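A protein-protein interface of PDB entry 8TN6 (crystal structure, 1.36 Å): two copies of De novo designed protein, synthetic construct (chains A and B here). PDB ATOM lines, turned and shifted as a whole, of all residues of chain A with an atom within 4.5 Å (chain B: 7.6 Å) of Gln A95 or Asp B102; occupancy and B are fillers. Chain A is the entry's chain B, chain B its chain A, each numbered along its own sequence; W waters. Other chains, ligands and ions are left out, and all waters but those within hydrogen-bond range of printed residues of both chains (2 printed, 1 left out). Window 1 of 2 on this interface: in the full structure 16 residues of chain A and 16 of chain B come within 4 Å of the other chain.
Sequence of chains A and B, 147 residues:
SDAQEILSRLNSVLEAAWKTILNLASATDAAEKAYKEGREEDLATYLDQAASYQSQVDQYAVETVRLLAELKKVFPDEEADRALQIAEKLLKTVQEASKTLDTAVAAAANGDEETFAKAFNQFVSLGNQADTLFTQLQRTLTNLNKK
Of the 10 printed residues of chain A, 3 touch a printed residue of chain B. Printed residues of chain B that touch a printed residue of chain A: Lys B99, Asp B102 and Ala B106. Among the printed residues, 4 pairs touch across the chains.
O of Ala B106 sits close to OD1 of Asn B110 (3.0 Å). The backbone carbonyl oxygen (O) of Lys B99 is in hydrogen-bond range of the side-chain hydroxyl (OG1) of Thr B103 (3.2 Å).
Lys A99 touches its own counterpart, Lys B99. Of the 4 pairs that touch across the chains among the printed residues, 1 has its exchanged pair printed and touching as well.
Among the printed residues, merely in contact across the chains: Gln A95 with Ala B106 (3.5 Å), Lys A99 with Lys B99 (3.6 Å) and Leu A91 with Ala B106 (3.8 Å).
Of the printed residues of chain B, Leu A91 touches Ala B106 (3.8 Å). Thr A93 touches none of the printed residues of chain B. Gln A95 touches two residues of chain B. Of the printed residues of chain A, Lys B99 touches Lys A99. Thr B100 touches none of the printed residues of chain A. Of the printed residues of chain A, Asp B102 touches Gln A95. The nearest residue of chain A that does not touch Asp B102 is Ser A98 (4.2 Å).
The backbone carbonyl oxygen of Asp B102 lies within hydrogen-bond range of the side-chain amide nitrogen of Gln A95.
Water W1 bridges the side-chain carboxylate of Asp B102 (2.7 Å) and the backbone carbonyl oxygen of Gln A95 (2.9 Å). Water W2 lies within hydrogen-bond range of NE2 of Gln A95 (2.7 Å) and OD1 of Asp B102 (2.9 Å).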
ATOM      1  N   ASP A  58      -0.094   7.414  19.722  1.00  0.00           N
ATOM      2  CA  ASP A  58      -0.181   7.812  18.323  1.00  0.00           C
ATOM      3  C   ASP A  58       0.382   9.207  18.143  1.00  0.00           C
ATOM      4  O   ASP A  58       1.122   9.452  17.193  1.00  0.00           O
ATOM      5  CB  ASP A  58      -1.618   7.750  17.828  1.00  0.00           C
ATOM      6  CG  ASP A  58      -2.183   6.350  17.804  1.00  0.00           C
ATOM      7  OD1 ASP A  58      -1.416   5.367  17.813  1.00  0.00           O
ATOM      8  OD2 ASP A  58      -3.424   6.247  17.690  1.00  0.00           O
ATOM      9  N   LEU A  91       4.820   4.346  13.361  1.00  0.00           N
ATOM     10  CA  LEU A  91       3.560   5.079  13.310  1.00  0.00           C
ATOM     11  C   LEU A  91       2.485   4.262  12.622  1.00  0.00           C
ATOM     12  O   LEU A  91       1.329   4.226  13.080  1.00  0.00           O
ATOM     13  CB  LEU A  91       3.780   6.430  12.624  1.00  0.00           C
ATOM     14  CG  LEU A  91       2.523   7.265  12.396  1.00  0.00           C
ATOM     15  CD1 LEU A  91       1.870   7.556  13.704  1.00  0.00           C
ATOM     16  CD2 LEU A  91       2.899   8.530  11.668  1.00  0.00           C
ATOM     17  N   LYS A  92       2.802   3.631  11.498  1.00  0.00           N
ATOM     18  CA  LYS A  92       1.811   2.829  10.800  1.00  0.00           C
ATOM     19  C   LYS A  92       1.287   1.727  11.718  1.00  0.00           C
ATOM     20  O   LYS A  92       0.082   1.451  11.778  1.00  0.00           O
ATOM     21  CB  LYS A  92       2.441   2.225   9.536  1.00  0.00           C
ATOM     22  CG  LYS A  92       1.494   1.430   8.690  1.00  0.00           C
ATOM     23  CD  LYS A  92       2.114   1.094   7.334  1.00  0.00           C
ATOM     24  CE  LYS A  92       1.296   0.016   6.614  1.00  0.00           C
ATOM     25  NZ  LYS A  92       1.618  -0.080   5.160  1.00  0.00           N
ATOM     26  N   THR A  93       2.195   1.104  12.468  1.00  0.00           N
ATOM     27  CA  THR A  93       1.811  -0.006  13.339  1.00  0.00           C
ATOM     28  C   THR A  93       0.961   0.477  14.506  1.00  0.00           C
ATOM     29  O   THR A  93      -0.037  -0.175  14.850  1.00  0.00           O
ATOM     30  CB  THR A  93       3.045  -0.738  13.823  1.00  0.00           C
ATOM     31  OG1 THR A  93       3.819  -1.159  12.698  1.00  0.00           O
ATOM     32  CG2 THR A  93       2.677  -1.962  14.625  1.00  0.00           C
ATOM     33  N   VAL A  94       1.319   1.603  15.133  1.00  0.00           N
ATOM     34  CA  VAL A  94       0.500   2.071  16.242  1.00  0.00           C
ATOM     35  C   VAL A  94      -0.855   2.529  15.746  1.00  0.00           C
ATOM     36  O   VAL A  94      -1.871   2.352  16.429  1.00  0.00           O
ATOM     37  CB  VAL A  94       1.206   3.099  17.141  1.00  0.00           C
ATOM     38  CG1 VAL A  94       2.524   2.536  17.654  1.00  0.00           C
ATOM     39  CG2 VAL A  94       1.446   4.413  16.448  1.00  0.00           C
ATOM     40  N   GLN A  95      -0.932   3.097  14.555  1.00  0.00           N
ATOM     41  CA  GLN A  95      -2.240   3.489  14.059  1.00  0.00           C
ATOM     42  C   GLN A  95      -3.069   2.265  13.723  1.00  0.00           C
ATOM     43  O   GLN A  95      -4.295   2.296  13.891  1.00  0.00           O
ATOM     44  CB  GLN A  95      -2.085   4.407  12.860  1.00  0.00           C
ATOM     45  CG  GLN A  95      -1.556   5.776  13.266  1.00  0.00           C
ATOM     46  CD  GLN A  95      -1.471   6.719  12.095  1.00  0.00           C
ATOM     47  OE1 GLN A  95      -1.257   6.280  10.955  1.00  0.00           O
ATOM     48  NE2 GLN A  95      -1.631   8.011  12.345  1.00  0.00           N
ATOM     49  N   GLU A  96      -2.440   1.196  13.247  1.00  0.00           N
ATOM     50  CA  GLU A  96      -3.169  -0.057  13.049  1.00  0.00           C
ATOM     51  C   GLU A  96      -3.684  -0.580  14.386  1.00  0.00           C
ATOM     52  O   GLU A  96      -4.807  -1.072  14.490  1.00  0.00           O
ATOM     53  CB  GLU A  96      -2.251  -1.110  12.436  1.00  0.00           C
ATOM     54  CG  GLU A  96      -2.060  -1.050  10.921  1.00  0.00           C
ATOM     55  CD  GLU A  96      -0.836  -1.848  10.395  1.00  0.00           C
ATOM     56  OE1 GLU A  96      -0.115  -2.500  11.188  1.00  0.00           O
ATOM     57  OE2 GLU A  96      -0.578  -1.804   9.164  1.00  0.00           O
ATOM     58  N   ALA A  97      -2.861  -0.478  15.420  1.00  0.00           N
ATOM     59  CA  ALA A  97      -3.294  -0.893  16.748  1.00  0.00           C
ATOM     60  C   ALA A  97      -4.455  -0.041  17.213  1.00  0.00           C
ATOM     61  O   ALA A  97      -5.427  -0.552  17.780  1.00  0.00           O
ATOM     62  CB  ALA A  97      -2.135  -0.805  17.735  1.00  0.00           C
ATOM     63  N   SER A  98      -4.425   1.254  16.928  1.00  0.00           N
ATOM     64  CA  SER A  98      -5.515   2.113  17.348  1.00  0.00           C
ATOM     65  C   SER A  98      -6.815   1.739  16.647  1.00  0.00           C
ATOM     66  O   SER A  98      -7.879   1.693  17.274  1.00  0.00           O
ATOM     67  CB  SER A  98      -5.162   3.563  17.019  1.00  0.00           C
ATOM     68  OG  SER A  98      -6.110   4.428  17.580  1.00  0.00           O
ATOM     69  N   LYS A  99      -6.767   1.429  15.358  1.00  0.00           N
ATOM     70  CA  LYS A  99      -7.963   1.038  14.619  1.00  0.00           C
ATOM     71  C   LYS A  99      -8.508  -0.277  15.160  1.00  0.00           C
ATOM     72  O   LYS A  99      -9.730  -0.465  15.293  1.00  0.00           O
ATOM     73  CB  LYS A  99      -7.590   0.910  13.127  1.00  0.00           C
ATOM     74  CG  LYS A  99      -8.653   0.244  12.229  1.00  0.00           C
ATOM     75  CD  LYS A  99      -8.083  -0.077  10.834  1.00  0.00           C
ATOM     76  CE  LYS A  99      -7.225  -1.341  10.858  1.00  0.00           C
ATOM     77  NZ  LYS A  99      -6.747  -1.743   9.498  1.00  0.00           N
ATOM     78  N   ALA B  51      -6.857  15.543  15.961  1.00  0.00           N
ATOM     79  CA  ALA B  51      -6.727  14.166  16.445  1.00  0.00           C
ATOM     80  C   ALA B  51      -7.166  14.066  17.900  1.00  0.00           C
ATOM     81  O   ALA B  51      -7.789  13.075  18.309  1.00  0.00           O
ATOM     82  CB  ALA B  51      -5.288  13.687  16.288  1.00  0.00           C
ATOM     83  N   GLN B  54     -10.932  14.318  17.990  1.00  0.00           N
ATOM     84  CA  GLN B  54     -11.519  13.104  17.461  1.00  0.00           C
ATOM     85  C   GLN B  54     -11.499  11.985  18.496  1.00  0.00           C
ATOM     86  O   GLN B  54     -12.467  11.233  18.619  1.00  0.00           O
ATOM     87  CB  GLN B  54     -10.765  12.679  16.214  1.00  0.00           C
ATOM     88  CG  GLN B  54     -11.319  11.443  15.566  1.00  0.00           C
ATOM     89  CD  GLN B  54     -12.665  11.692  14.960  1.00  0.00           C
ATOM     90  OE1 GLN B  54     -12.776  12.429  13.998  1.00  0.00           O
ATOM     91  NE2 GLN B  54     -13.716  11.144  15.541  1.00  0.00           N
ATOM     92  N   SER B  55     -10.414  11.852  19.255  1.00  0.00           N
ATOM     93  CA  SER B  55     -10.370  10.795  20.267  1.00  0.00           C
ATOM     94  C   SER B  55     -11.424  11.037  21.330  1.00  0.00           C
ATOM     95  O   SER B  55     -12.041  10.089  21.833  1.00  0.00           O
ATOM     96  CB  SER B  55      -8.963  10.742  20.851  1.00  0.00           C
ATOM     97  OG  SER B  55      -8.104   9.977  20.010  1.00  0.00           O
ATOM     98  N   GLN B  95     -15.675   6.193  14.341  1.00  0.00           N
ATOM     99  CA  GLN B  95     -14.440   5.428  14.312  1.00  0.00           C
ATOM    100  C   GLN B  95     -13.878   5.336  12.898  1.00  0.00           C
ATOM    101  O   GLN B  95     -12.660   5.315  12.730  1.00  0.00           O
ATOM    102  CB  GLN B  95     -14.665   4.040  14.907  1.00  0.00           C
ATOM    103  CG  GLN B  95     -14.937   4.082  16.398  1.00  0.00           C
ATOM    104  CD  GLN B  95     -15.080   2.710  17.010  1.00  0.00           C
ATOM    105  OE1 GLN B  95     -15.539   1.784  16.348  1.00  0.00           O
ATOM    106  NE2 GLN B  95     -14.696   2.580  18.276  1.00  0.00           N
ATOM    107  N   GLU B  96     -14.722   5.305  11.872  1.00  0.00           N
ATOM    108  CA  GLU B  96     -14.184   5.381  10.517  1.00  0.00           C
ATOM    109  C   GLU B  96     -13.535   6.737  10.259  1.00  0.00           C
ATOM    110  O   GLU B  96     -12.470   6.804   9.636  1.00  0.00           O
ATOM    111  CB  GLU B  96     -15.285   5.127   9.499  1.00  0.00           C
ATOM    112  CG  GLU B  96     -14.782   4.881   8.097  1.00  0.00           C
ATOM    113  CD  GLU B  96     -15.909   4.614   7.120  1.00  0.00           C
ATOM    114  OE1 GLU B  96     -17.078   4.482   7.572  1.00  0.00           O
ATOM    115  OE2 GLU B  96     -15.618   4.533   5.901  1.00  0.00           O
ATOM    116  N   ALA B  97     -14.158   7.816  10.744  1.00  0.00           N
ATOM    117  CA  ALA B  97     -13.536   9.138  10.662  1.00  0.00           C
ATOM    118  C   ALA B  97     -12.183   9.125  11.360  1.00  0.00           C
ATOM    119  O   ALA B  97     -11.209   9.672  10.853  1.00  0.00           O
ATOM    120  CB  ALA B  97     -14.458  10.193  11.268  1.00  0.00           C
ATOM    121  N   SER B  98     -12.093   8.508  12.529  1.00  0.00           N
ATOM    122  CA  SER B  98     -10.834   8.461  13.258  1.00  0.00           C
ATOM    123  C   SER B  98      -9.751   7.743  12.465  1.00  0.00           C
ATOM    124  O   SER B  98      -8.602   8.193  12.419  1.00  0.00           O
ATOM    125  CB  SER B  98     -11.080   7.766  14.601  1.00  0.00           C
ATOM    126  OG  SER B  98     -10.028   8.068  15.492  1.00  0.00           O
ATOM    127  N   LYS B  99     -10.090   6.595  11.866  1.00  0.00           N
ATOM    128  CA  LYS B  99      -9.125   5.850  11.058  1.00  0.00           C
ATOM    129  C   LYS B  99      -8.672   6.703   9.883  1.00  0.00           C
ATOM    130  O   LYS B  99      -7.497   6.692   9.504  1.00  0.00           O
ATOM    131  CB  LYS B  99      -9.805   4.560  10.546  1.00  0.00           C
ATOM    132  CG  LYS B  99      -9.012   3.770   9.505  1.00  0.00           C
ATOM    133  CD  LYS B  99      -9.771   2.540   8.996  1.00  0.00           C
ATOM    134  CE  LYS B  99     -10.753   2.918   7.899  1.00  0.00           C
ATOM    135  NZ  LYS B  99     -11.191   1.726   7.112  1.00  0.00           N
ATOM    136  N   THR B 100      -9.609   7.442   9.296  1.00  0.00           N
ATOM    137  CA  THR B 100      -9.285   8.267   8.130  1.00  0.00           C
ATOM    138  C   THR B 100      -8.418   9.442   8.523  1.00  0.00           C
ATOM    139  O   THR B 100      -7.446   9.755   7.827  1.00  0.00           O
ATOM    140  CB  THR B 100     -10.579   8.716   7.493  1.00  0.00           C
ATOM    141  OG1 THR B 100     -11.344   7.559   7.136  1.00  0.00           O
ATOM    142  CG2 THR B 100     -10.313   9.538   6.263  1.00  0.00           C
ATOM    143  N   LEU B 101      -8.714  10.068   9.663  1.00  0.00           N
ATOM    144  CA  LEU B 101      -7.841  11.121  10.163  1.00  0.00           C
ATOM    145  C   LEU B 101      -6.446  10.588  10.431  1.00  0.00           C
ATOM    146  O   LEU B 101      -5.447  11.261  10.137  1.00  0.00           O
ATOM    147  CB  LEU B 101      -8.457  11.749  11.404  1.00  0.00           C
ATOM    148  CG  LEU B 101      -7.697  12.911  12.001  1.00  0.00           C
ATOM    149  CD1 LEU B 101      -7.619  14.078  10.997  1.00  0.00           C
ATOM    150  CD2 LEU B 101      -8.346  13.358  13.251  1.00  0.00           C
ATOM    151  N   ASP B 102      -6.337   9.374  10.969  1.00  0.00           N
ATOM    152  CA  ASP B 102      -5.018   8.807  11.219  1.00  0.00           C
ATOM    153  C   ASP B 102      -4.227   8.733   9.917  1.00  0.00           C
ATOM    154  O   ASP B 102      -3.045   9.084   9.865  1.00  0.00           O
ATOM    155  CB  ASP B 102      -5.157   7.387  11.813  1.00  0.00           C
ATOM    156  CG  ASP B 102      -5.300   7.363  13.318  1.00  0.00           C
ATOM    157  OD1 ASP B 102      -5.167   8.410  13.994  1.00  0.00           O
ATOM    158  OD2 ASP B 102      -5.587   6.251  13.828  1.00  0.00           O
ATOM    159  N   THR B 103      -4.872   8.278   8.846  1.00  0.00           N
ATOM    160  CA  THR B 103      -4.228   8.229   7.535  1.00  0.00           C
ATOM    161  C   THR B 103      -3.784   9.613   7.095  1.00  0.00           C
ATOM    162  O   THR B 103      -2.660   9.790   6.613  1.00  0.00           O
ATOM    163  CB  THR B 103      -5.213   7.636   6.534  1.00  0.00           C
ATOM    164  OG1 THR B 103      -5.543   6.292   6.938  1.00  0.00           O
ATOM    165  CG2 THR B 103      -4.659   7.608   5.136  1.00  0.00           C
ATOM    166  N   ALA B 104      -4.640  10.612   7.283  1.00  0.00           N
ATOM    167  CA  ALA B 104      -4.277  11.966   6.871  1.00  0.00           C
ATOM    168  C   ALA B 104      -3.104  12.496   7.685  1.00  0.00           C
ATOM    169  O   ALA B 104      -2.159  13.068   7.128  1.00  0.00           O
ATOM    170  CB  ALA B 104      -5.487  12.883   7.008  1.00  0.00           C
ATOM    171  N   VAL B 105      -3.125  12.297   9.002  1.00  0.00           N
ATOM    172  CA  VAL B 105      -2.075  12.799   9.862  1.00  0.00           C
ATOM    173  C   VAL B 105      -0.745  12.139   9.534  1.00  0.00           C
ATOM    174  O   VAL B 105       0.304  12.794   9.519  1.00  0.00           O
ATOM    175  CB  VAL B 105      -2.450  12.597  11.350  1.00  0.00           C
ATOM    176  CG1 VAL B 105      -1.262  12.844  12.225  1.00  0.00           C
ATOM    177  CG2 VAL B 105      -3.601  13.466  11.722  1.00  0.00           C
ATOM    178  N   ALA B 106      -0.751  10.826   9.295  1.00  0.00           N
ATOM    179  CA  ALA B 106       0.479  10.158   8.918  1.00  0.00           C
ATOM    180  C   ALA B 106       0.982  10.665   7.582  1.00  0.00           C
ATOM    181  O   ALA B 106       2.183  10.866   7.419  1.00  0.00           O
ATOM    182  CB  ALA B 106       0.257   8.645   8.885  1.00  0.00           C
ATOM    183  N   ALA B 107       0.076  10.880   6.626  1.00  0.00           N
ATOM    184  CA  ALA B 107       0.491  11.352   5.307  1.00  0.00           C
ATOM    185  C   ALA B 107       1.104  12.742   5.397  1.00  0.00           C
ATOM    186  O   ALA B 107       2.110  13.030   4.734  1.00  0.00           O
ATOM    187  CB  ALA B 107      -0.702  11.357   4.365  1.00  0.00           C
ATOM    188  N   ALA B 108       0.522  13.627   6.202  1.00  0.00           N
ATOM    189  CA  ALA B 108       1.084  14.960   6.376  1.00  0.00           C
ATOM    190  C   ALA B 108       2.442  14.890   7.060  1.00  0.00           C
ATOM    191  O   ALA B 108       3.369  15.625   6.695  1.00  0.00           O
ATOM    192  CB  ALA B 108       0.111  15.821   7.172  1.00  0.00           C
ATOM    193  N   ASN B 110       4.522  12.327   6.882  1.00  0.00           N
ATOM    194  CA  ASN B 110       5.392  11.643   5.928  1.00  0.00           C
ATOM    195  C   ASN B 110       5.630  12.478   4.670  1.00  0.00           C
ATOM    196  O   ASN B 110       6.417  12.053   3.812  1.00  0.00           O
ATOM    197  CB  ASN B 110       4.762  10.305   5.476  1.00  0.00           C
ATOM    198  CG  ASN B 110       4.978   9.153   6.463  1.00  0.00           C
ATOM    199  OD1 ASN B 110       4.649   9.228   7.657  1.00  0.00           O
ATOM    200  ND2 ASN B 110       5.497   8.042   5.939  1.00  0.00           N
ATOM    201  N   ALA B 119      -7.446  11.699   1.999  1.00  0.00           N
ATOM    202  CA  ALA B 119      -7.957  11.248   3.286  1.00  0.00           C
ATOM    203  C   ALA B 119      -8.674  12.374   4.005  1.00  0.00           C
ATOM    204  O   ALA B 119      -9.695  12.148   4.662  1.00  0.00           O
ATOM    205  CB  ALA B 119      -6.799  10.757   4.151  1.00  0.00           C
ATOM    206  N   PHE B 123     -12.379  12.429   5.328  1.00  0.00           N
ATOM    207  CA  PHE B 123     -12.659  12.741   6.729  1.00  0.00           C
ATOM    208  C   PHE B 123     -13.842  13.684   6.859  1.00  0.00           C
ATOM    209  O   PHE B 123     -14.756  13.463   7.658  1.00  0.00           O
ATOM    210  CB  PHE B 123     -11.399  13.330   7.335  1.00  0.00           C
ATOM    211  CG  PHE B 123     -11.544  13.705   8.792  1.00  0.00           C
ATOM    212  CD1 PHE B 123     -11.684  12.747   9.760  1.00  0.00           C
ATOM    213  CD2 PHE B 123     -11.585  15.030   9.162  1.00  0.00           C
ATOM    214  CE1 PHE B 123     -11.830  13.127  11.092  1.00  0.00           C
ATOM    215  CE2 PHE B 123     -11.707  15.399  10.492  1.00  0.00           C
ATOM    216  CZ  PHE B 123     -11.849  14.430  11.440  1.00  0.00           C
HETATM  217  O   HOH W   1      -5.940   4.071  12.306  1.00  0.00           O
HETATM  218  O   HOH W   2      -2.446   8.948  14.734  1.00  0.00           O
